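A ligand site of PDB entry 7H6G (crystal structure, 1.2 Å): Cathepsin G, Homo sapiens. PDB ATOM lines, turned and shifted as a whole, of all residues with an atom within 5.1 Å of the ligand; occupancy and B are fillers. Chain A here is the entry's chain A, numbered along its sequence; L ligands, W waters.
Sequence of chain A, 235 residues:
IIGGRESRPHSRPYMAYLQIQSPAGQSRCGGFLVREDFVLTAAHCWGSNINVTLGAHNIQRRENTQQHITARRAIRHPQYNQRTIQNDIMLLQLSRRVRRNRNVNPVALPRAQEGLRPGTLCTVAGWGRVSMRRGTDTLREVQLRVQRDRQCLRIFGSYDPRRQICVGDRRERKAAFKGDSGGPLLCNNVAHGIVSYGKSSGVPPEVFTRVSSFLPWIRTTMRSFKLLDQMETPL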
ATOM      1  N   ILE A  20      10.590  17.130   4.113  1.00  0.00           N
ATOM      2  CA  ILE A  20      11.249  18.438   4.029  1.00  0.00           C
ATOM      3  C   ILE A  20      12.471  18.419   3.167  1.00  0.00           C
ATOM      4  O   ILE A  20      13.462  17.751   3.470  1.00  0.00           O
ATOM      5  CB  ILE A  20      11.613  18.988   5.387  1.00  0.00           C
ATOM      6  CG1 ILE A  20      10.350  19.092   6.251  1.00  0.00           C
ATOM      7  CG2 ILE A  20      12.203  20.369   5.238  1.00  0.00           C
ATOM      8  CD1 ILE A  20      10.346  18.148   7.340  1.00  0.00           C
ATOM      9  N   SER A  27      14.485  15.222   4.637  1.00  0.00           N
ATOM     10  CA  SER A  27      14.353  14.834   6.019  1.00  0.00           C
ATOM     11  C   SER A  27      12.869  14.663   6.324  1.00  0.00           C
ATOM     12  O   SER A  27      12.003  15.089   5.560  1.00  0.00           O
ATOM     13  CB  SER A  27      14.953  15.892   6.958  1.00  0.00           C
ATOM     14  OG  SER A  27      16.356  16.013   6.740  1.00  0.00           O
ATOM     15  N   ARG A  28      12.588  14.039   7.457  1.00  0.00           N
ATOM     16  CA  ARG A  28      11.263  13.685   7.858  1.00  0.00           C
ATOM     17  C   ARG A  28      10.910  14.405   9.148  1.00  0.00           C
ATOM     18  O   ARG A  28      11.709  14.487  10.075  1.00  0.00           O
ATOM     19  CB  ARG A  28      11.317  12.187   8.136  1.00  0.00           C
ATOM     20  CG  ARG A  28      10.066  11.592   8.657  1.00  0.00           C
ATOM     21  CD  ARG A  28      10.126  10.062   8.738  1.00  0.00           C
ATOM     22  NE  ARG A  28      10.383   9.444   7.439  1.00  0.00           N
ATOM     23  CZ  ARG A  28      10.142   8.172   7.162  1.00  0.00           C
ATOM     24  NH1 ARG A  28       9.653   7.371   8.081  1.00  0.00           N
ATOM     25  NH2 ARG A  28      10.406   7.697   5.950  1.00  0.00           N
ATOM     26  N   CYS A  29       9.657  14.834   9.216  1.00  0.00           N
ATOM     27  CA  CYS A  29       9.079  15.329  10.462  1.00  0.00           C
ATOM     28  C   CYS A  29       7.645  14.905  10.532  1.00  0.00           C
ATOM     29  O   CYS A  29       7.038  14.538   9.510  1.00  0.00           O
ATOM     30  CB  CYS A  29       9.161  16.846  10.565  1.00  0.00           C
ATOM     31  SG  CYS A  29      10.771  17.506  11.023  1.00  0.00           S
ATOM     32  N   HIS A  44      12.244  23.801  13.339  1.00  0.00           N
ATOM     33  CA  HIS A  44      13.461  23.239  12.770  1.00  0.00           C
ATOM     34  C   HIS A  44      13.198  22.314  11.593  1.00  0.00           C
ATOM     35  O   HIS A  44      14.121  21.892  10.895  1.00  0.00           O
ATOM     36  CB  HIS A  44      14.347  22.576  13.832  1.00  0.00           C
ATOM     37  CG  HIS A  44      13.966  21.184  14.194  1.00  0.00           C
ATOM     38  ND1 HIS A  44      13.320  20.875  15.378  1.00  0.00           N
ATOM     39  CD2 HIS A  44      14.256  19.999  13.609  1.00  0.00           C
ATOM     40  CE1 HIS A  44      13.229  19.557  15.481  1.00  0.00           C
ATOM     41  NE2 HIS A  44      13.771  19.009  14.421  1.00  0.00           N
ATOM     42  N   CYS A  45      11.926  22.001  11.386  1.00  0.00           N
ATOM     43  CA  CYS A  45      11.505  21.184  10.264  1.00  0.00           C
ATOM     44  C   CYS A  45      11.299  22.056   9.026  1.00  0.00           C
ATOM     45  O   CYS A  45      10.789  21.598   8.036  1.00  0.00           O
ATOM     46  CB  CYS A  45      10.207  20.468  10.607  1.00  0.00           C
ATOM     47  SG  CYS A  45      10.346  19.261  11.959  1.00  0.00           S
ATOM     48  N   TRP A  46      11.618  23.337   9.118  1.00  0.00           N
ATOM     49  CA  TRP A  46      11.505  24.181   7.941  1.00  0.00           C
ATOM     50  C   TRP A  46      12.431  23.688   6.799  1.00  0.00           C
ATOM     51  O   TRP A  46      13.530  23.219   7.002  1.00  0.00           O
ATOM     52  CB  TRP A  46      11.806  25.622   8.311  1.00  0.00           C
ATOM     53  CG  TRP A  46      11.584  26.550   7.190  1.00  0.00           C
ATOM     54  CD1 TRP A  46      10.464  27.235   6.911  1.00  0.00           C
ATOM     55  CD2 TRP A  46      12.528  26.906   6.176  1.00  0.00           C
ATOM     56  NE1 TRP A  46      10.616  27.959   5.769  1.00  0.00           N
ATOM     57  CE2 TRP A  46      11.879  27.769   5.299  1.00  0.00           C
ATOM     58  CE3 TRP A  46      13.843  26.532   5.902  1.00  0.00           C
ATOM     59  CZ2 TRP A  46      12.509  28.301   4.166  1.00  0.00           C
ATOM     60  CZ3 TRP A  46      14.452  27.049   4.784  1.00  0.00           C
ATOM     61  CH2 TRP A  46      13.789  27.927   3.946  1.00  0.00           C
ATOM     62  N   ILE A  85      17.561  26.175  19.865  1.00  0.00           N
ATOM     63  CA  ILE A  85      16.329  25.455  19.548  1.00  0.00           C
ATOM     64  C   ILE A  85      15.167  25.978  20.359  1.00  0.00           C
ATOM     65  O   ILE A  85      14.094  25.355  20.370  1.00  0.00           O
ATOM     66  CB  ILE A  85      16.474  23.901  19.609  1.00  0.00           C
ATOM     67  CG1 ILE A  85      17.894  23.445  19.206  1.00  0.00           C
ATOM     68  CG2 ILE A  85      15.485  23.250  18.644  1.00  0.00           C
ATOM     69  CD1 ILE A  85      18.137  21.956  19.240  1.00  0.00           C
ATOM     70  N   ASP A  88      10.669  26.462  19.145  1.00  0.00           N
ATOM     71  CA  ASP A  88      10.664  25.523  18.049  1.00  0.00           C
ATOM     72  C   ASP A  88       9.242  25.151  17.664  1.00  0.00           C
ATOM     73  O   ASP A  88       8.733  24.079  17.967  1.00  0.00           O
ATOM     74  CB  ASP A  88      11.475  24.261  18.425  1.00  0.00           C
ATOM     75  CG  ASP A  88      11.797  23.383  17.235  1.00  0.00           C
ATOM     76  OD1 ASP A  88      11.650  23.841  16.092  1.00  0.00           O
ATOM     77  OD2 ASP A  88      12.235  22.231  17.473  1.00  0.00           O
ATOM     78  N   ALA A 176      10.376   9.636  21.716  1.00  0.00           N
ATOM     79  CA  ALA A 176      10.339  10.126  20.337  1.00  0.00           C
ATOM     80  C   ALA A 176      11.789  10.235  19.868  1.00  0.00           C
ATOM     81  O   ALA A 176      12.703  10.462  20.664  1.00  0.00           O
ATOM     82  CB  ALA A 176       9.644  11.456  20.280  1.00  0.00           C
ATOM     83  N   PHE A 177      12.032  10.100  18.571  1.00  0.00           N
ATOM     84  CA  PHE A 177      13.397  10.203  18.087  1.00  0.00           C
ATOM     85  C   PHE A 177      13.402  10.879  16.704  1.00  0.00           C
ATOM     86  O   PHE A 177      12.402  11.446  16.276  1.00  0.00           O
ATOM     87  CB  PHE A 177      14.112   8.826  18.144  1.00  0.00           C
ATOM     88  CG  PHE A 177      15.610   8.929  18.018  1.00  0.00           C
ATOM     89  CD1 PHE A 177      16.325   9.735  18.870  1.00  0.00           C
ATOM     90  CD2 PHE A 177      16.320   8.217  17.064  1.00  0.00           C
ATOM     91  CE1 PHE A 177      17.690   9.866  18.750  1.00  0.00           C
ATOM     92  CE2 PHE A 177      17.682   8.371  16.948  1.00  0.00           C
ATOM     93  CZ  PHE A 177      18.351   9.200  17.807  1.00  0.00           C
ATOM     94  N   LYS A 178      14.555  10.889  16.048  1.00  0.00           N
ATOM     95  CA  LYS A 178      14.707  11.531  14.760  1.00  0.00           C
ATOM     96  C   LYS A 178      13.611  11.088  13.821  1.00  0.00           C
ATOM     97  O   LYS A 178      13.371   9.899  13.659  1.00  0.00           O
ATOM     98  CB  LYS A 178      16.069  11.208  14.157  1.00  0.00           C
ATOM     99  CG  LYS A 178      17.235  11.757  14.934  1.00  0.00           C
ATOM    100  CD  LYS A 178      18.515  11.250  14.340  1.00  0.00           C
ATOM    101  CE  LYS A 178      19.756  11.851  14.981  1.00  0.00           C
ATOM    102  NZ  LYS A 178      20.985  11.192  14.461  1.00  0.00           N
ATOM    103  N   GLY A 179      12.995  12.045  13.167  1.00  0.00           N
ATOM    104  CA  GLY A 179      11.862  11.831  12.276  1.00  0.00           C
ATOM    105  C   GLY A 179      10.520  12.085  12.928  1.00  0.00           C
ATOM    106  O   GLY A 179       9.515  12.228  12.223  1.00  0.00           O
ATOM    107  N   ASP A 180      10.510  12.151  14.254  1.00  0.00           N
ATOM    108  CA  ASP A 180       9.302  12.427  15.012  1.00  0.00           C
ATOM    109  C   ASP A 180       9.090  13.904  15.369  1.00  0.00           C
ATOM    110  O   ASP A 180       8.024  14.255  15.885  1.00  0.00           O
ATOM    111  CB  ASP A 180       9.257  11.618  16.332  1.00  0.00           C
ATOM    112  CG  ASP A 180       9.149  10.130  16.135  1.00  0.00           C
ATOM    113  OD1 ASP A 180       8.332   9.708  15.274  1.00  0.00           O
ATOM    114  OD2 ASP A 180       9.862   9.394  16.876  1.00  0.00           O
ATOM    115  N   SER A 181      10.097  14.746  15.160  1.00  0.00           N
ATOM    116  CA  SER A 181       9.965  16.148  15.524  1.00  0.00           C
ATOM    117  C   SER A 181       8.736  16.711  14.866  1.00  0.00           C
ATOM    118  O   SER A 181       8.454  16.406  13.719  1.00  0.00           O
ATOM    119  CB  SER A 181      11.166  16.966  15.108  1.00  0.00           C
ATOM    120  OG  SER A 181      12.371  16.534  15.747  1.00  0.00           O
ATOM    121  N   VAL A 195       6.878  17.566  19.652  1.00  0.00           N
ATOM    122  CA  VAL A 195       8.228  16.961  19.745  1.00  0.00           C
ATOM    123  C   VAL A 195       9.241  17.970  19.212  1.00  0.00           C
ATOM    124  O   VAL A 195       9.091  18.470  18.085  1.00  0.00           O
ATOM    125  CB  VAL A 195       8.367  15.696  18.905  1.00  0.00           C
ATOM    126  CG1 VAL A 195       9.757  15.121  19.020  1.00  0.00           C
ATOM    127  CG2 VAL A 195       7.322  14.645  19.296  1.00  0.00           C
ATOM    128  N   SER A 196      10.289  18.272  19.982  1.00  0.00           N
ATOM    129  CA  SER A 196      11.379  19.123  19.512  1.00  0.00           C
ATOM    130  C   SER A 196      12.638  18.306  19.316  1.00  0.00           C
ATOM    131  O   SER A 196      12.996  18.001  18.164  1.00  0.00           O
ATOM    132  CB  SER A 196      11.555  20.336  20.409  1.00  0.00           C
ATOM    133  OG  SER A 196      12.548  21.184  19.887  1.00  0.00           O
ATOM    134  N   TYR A 197      13.298  17.918  20.388  1.00  0.00           N
ATOM    135  CA  TYR A 197      14.572  17.201  20.272  1.00  0.00           C
ATOM    136  C   TYR A 197      14.898  16.491  21.561  1.00  0.00           C
ATOM    137  O   TYR A 197      14.316  16.749  22.592  1.00  0.00           O
ATOM    138  CB  TYR A 197      15.722  18.138  19.865  1.00  0.00           C
ATOM    139  CG  TYR A 197      16.103  19.091  20.952  1.00  0.00           C
ATOM    140  CD1 TYR A 197      15.431  20.267  21.167  1.00  0.00           C
ATOM    141  CD2 TYR A 197      17.176  18.802  21.777  1.00  0.00           C
ATOM    142  CE1 TYR A 197      15.774  21.107  22.181  1.00  0.00           C
ATOM    143  CE2 TYR A 197      17.532  19.628  22.806  1.00  0.00           C
ATOM    144  CZ  TYR A 197      16.820  20.794  23.013  1.00  0.00           C
ATOM    145  OH  TYR A 197      17.184  21.649  24.042  1.00  0.00           O
ATOM    146  N   GLY A 198      15.910  15.664  21.479  1.00  0.00           N
ATOM    147  CA  GLY A 198      16.510  15.010  22.628  1.00  0.00           C
ATOM    148  C   GLY A 198      17.968  14.741  22.359  1.00  0.00           C
ATOM    149  O   GLY A 198      18.559  15.293  21.432  1.00  0.00           O
ATOM    150  N   LYS A 199      18.558  13.863  23.180  1.00  0.00           N
ATOM    151  CA  LYS A 199      19.927  13.432  22.946  1.00  0.00           C
ATOM    152  C   LYS A 199      20.044  12.594  21.681  1.00  0.00           C
ATOM    153  O   LYS A 199      19.124  11.856  21.299  1.00  0.00           O
ATOM    154  CB  LYS A 199      20.411  12.615  24.148  1.00  0.00           C
ATOM    155  CG  LYS A 199      20.494  13.415  25.447  1.00  0.00           C
ATOM    156  CD  LYS A 199      21.662  14.364  25.438  1.00  0.00           C
ATOM    157  CE  LYS A 199      21.825  15.130  26.739  1.00  0.00           C
ATOM    158  NZ  LYS A 199      23.034  16.016  26.710  1.00  0.00           N
ATOM    159  N   SER A 200      21.208  12.642  21.057  1.00  0.00           N
ATOM    160  CA  SER A 200      21.464  11.846  19.867  1.00  0.00           C
ATOM    161  C   SER A 200      21.461  10.334  20.120  1.00  0.00           C
ATOM    162  O   SER A 200      21.323   9.537  19.180  1.00  0.00           O
ATOM    163  CB  SER A 200      22.762  12.293  19.230  1.00  0.00           C
ATOM    164  OG  SER A 200      22.654  13.620  18.792  1.00  0.00           O
ATOM    165  N   GLU A 206      13.554  14.095  27.036  1.00  0.00           N
ATOM    166  CA  GLU A 206      13.665  14.905  25.832  1.00  0.00           C
ATOM    167  C   GLU A 206      12.763  16.117  25.939  1.00  0.00           C
ATOM    168  O   GLU A 206      11.968  16.240  26.858  1.00  0.00           O
ATOM    169  CB  GLU A 206      13.389  14.109  24.578  1.00  0.00           C
ATOM    170  CG  GLU A 206      12.054  13.563  24.506  1.00  0.00           C
ATOM    171  CD  GLU A 206      11.928  12.440  23.495  1.00  0.00           C
ATOM    172  OE1 GLU A 206      12.840  12.262  22.636  1.00  0.00           O
ATOM    173  OE2 GLU A 206      10.911  11.759  23.555  1.00  0.00           O
HETATM  174  C1  LIG L   1      16.881  15.904  13.618  1.00  0.00           C
HETATM  175  C2  LIG L   1      16.563  15.511  16.051  1.00  0.00           C
HETATM  176  C3  LIG L   1      15.686  16.009  12.995  1.00  0.00           C
HETATM  177  C4  LIG L   1      17.819  15.416  12.654  1.00  0.00           C
HETATM  178  C5  LIG L   1      15.814  15.637  11.543  1.00  0.00           C
HETATM  179  C6  LIG L   1      16.087  14.261  17.926  1.00  0.00           C
HETATM  180  C7  LIG L   1      13.686  14.300  17.769  1.00  0.00           C
HETATM  181  C8  LIG L   1      16.063  13.479  19.071  1.00  0.00           C
HETATM  182  C9  LIG L   1      17.187  17.751  15.230  1.00  0.00           C
HETATM  183  O1  LIG L   1      14.543  16.413  13.500  1.00  0.00           O
HETATM  184  O2  LIG L   1      19.378  18.624  18.910  1.00  0.00           O
HETATM  185  C10 LIG L   1      14.808  13.155  19.579  1.00  0.00           C
HETATM  186  C11 LIG L   1      15.031  14.411  11.136  1.00  0.00           C
HETATM  187  C12 LIG L   1      15.527  16.864  10.699  1.00  0.00           C
HETATM  188  C13 LIG L   1      16.483  17.825  10.435  1.00  0.00           C
HETATM  189  C14 LIG L   1      16.177  18.942   9.660  1.00  0.00           C
HETATM  190  C15 LIG L   1      14.895  19.134   9.150  1.00  0.00           C
HETATM  191  C16 LIG L   1      13.915  18.190   9.424  1.00  0.00           C
HETATM  192  C17 LIG L   1      14.232  17.060  10.183  1.00  0.00           C
HETATM  193  O3  LIG L   1      17.205  15.251  11.454  1.00  0.00           O
HETATM  194  O4  LIG L   1      18.991  15.165  12.792  1.00  0.00           O
HETATM  195  C18 LIG L   1      17.299  16.250  15.010  1.00  0.00           C
HETATM  196  C19 LIG L   1      17.802  18.599  14.315  1.00  0.00           C
HETATM  197  C20 LIG L   1      17.763  19.974  14.475  1.00  0.00           C
HETATM  198  C21 LIG L   1      17.082  20.531  15.540  1.00  0.00           C
HETATM  199  C22 LIG L   1      16.454  19.708  16.462  1.00  0.00           C
HETATM  200  C23 LIG L   1      16.493  18.333  16.302  1.00  0.00           C
HETATM  201  N1  LIG L   1      15.237  15.399  16.171  1.00  0.00           N
HETATM  202  C24 LIG L   1      14.921  14.671  17.262  1.00  0.00           C
HETATM  203  C25 LIG L   1      13.637  13.556  18.937  1.00  0.00           C
HETATM  204  F1  LIG L   1      12.427  13.250  19.432  1.00  0.00           F
HETATM  205  C26 LIG L   1      17.185  14.799  17.155  1.00  0.00           C
HETATM  206  C27 LIG L   1      18.647  14.649  17.460  1.00  0.00           C
HETATM  207  C28 LIG L   1      19.081  15.913  18.296  1.00  0.00           C
HETATM  208  N2  LIG L   1      19.819  16.921  17.527  1.00  0.00           N
HETATM  209  C29 LIG L   1      19.886  18.191  17.906  1.00  0.00           C
HETATM  210  C30 LIG L   1      20.669  19.103  17.005  1.00  0.00           C
HETATM  211  O   HOH W   1      16.359  11.536  22.022  1.00  0.00           O
HETATM  212  O   HOH W   2      12.310  14.831  13.038  1.00  0.00           O
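O of Ala 176 sits close to F1 of the ligand.
The backbone NH (N) of Phe 177 sits close to a fluorine (F1) of the ligand, 3.3 Å away.
OE1 of Glu 206 lies close to F1 of the ligand, 3.4 Å away.
Ser 27 touches the ligand.
O of Arg 28 touches C11 of the ligand (3.5 Å).
SG of Cys 29 touches C17 of the ligand (3.6 Å).
CA of Cys 45 touches C16 of the ligand, 3.9 Å away.
Ile 85 touches the ligand.
Lys 178 touches the ligand.
Gly 179 touches the ligand (N to C11, 3.7 Å).
CG1 of Val 195 touches F1 of the ligand (3.3 Å).
Ser 196 touches the ligand (O to C7, 3.8 Å).
Tyr 197 touches the ligand.
O of Gly 198 touches C28 of the ligand, 3.2 Å away.
Hydrophobic or aromatic side chains that line the ligand: His 44, Ile 85, Ala 176, Phe 177, Val 195 and Tyr 197.
The nearest printed residue that does not touch the ligand is Lys 199 (4.1 Å).
An oxygen (O1) of the ligand lies within hydrogen-bond range of a ring nitrogen (NE2) of His 44 (2.9 Å).
N1 of the ligand is in hydrogen-bond range of OG of Ser 181, at 3.1 Å.
NE2 of His 44 lies within hydrogen-bond range of OG of Ser 181 (3.1 Å).
The side-chain carboxylate of Asp 88 lies within hydrogen-bond range of a ring nitrogen (ND1) of His 44 (2.7 Å).
OE2 of Glu 206 sits at hydrogen-bond distance from N of Ala 176, 2.9 Å away.
OG of Ser 181 is in hydrogen-bond range of O of Ser 196 (2.9 Å).
The side-chain carboxylate (OD2) of Asp 180 lies within hydrogen-bond range of the backbone NH (N) of Phe 177 (2.8 Å).
O of Ser 27 is in hydrogen-bond range of N of Ile 20 (2.9 Å).
The side-chain sulfur (SG) of Cys 29 is disulfide-bonded to the side-chain sulfur (SG) of Cys 45 (2.0 Å).
OG of Ser 196 lies within hydrogen-bond range of OD2 of Asp 88.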
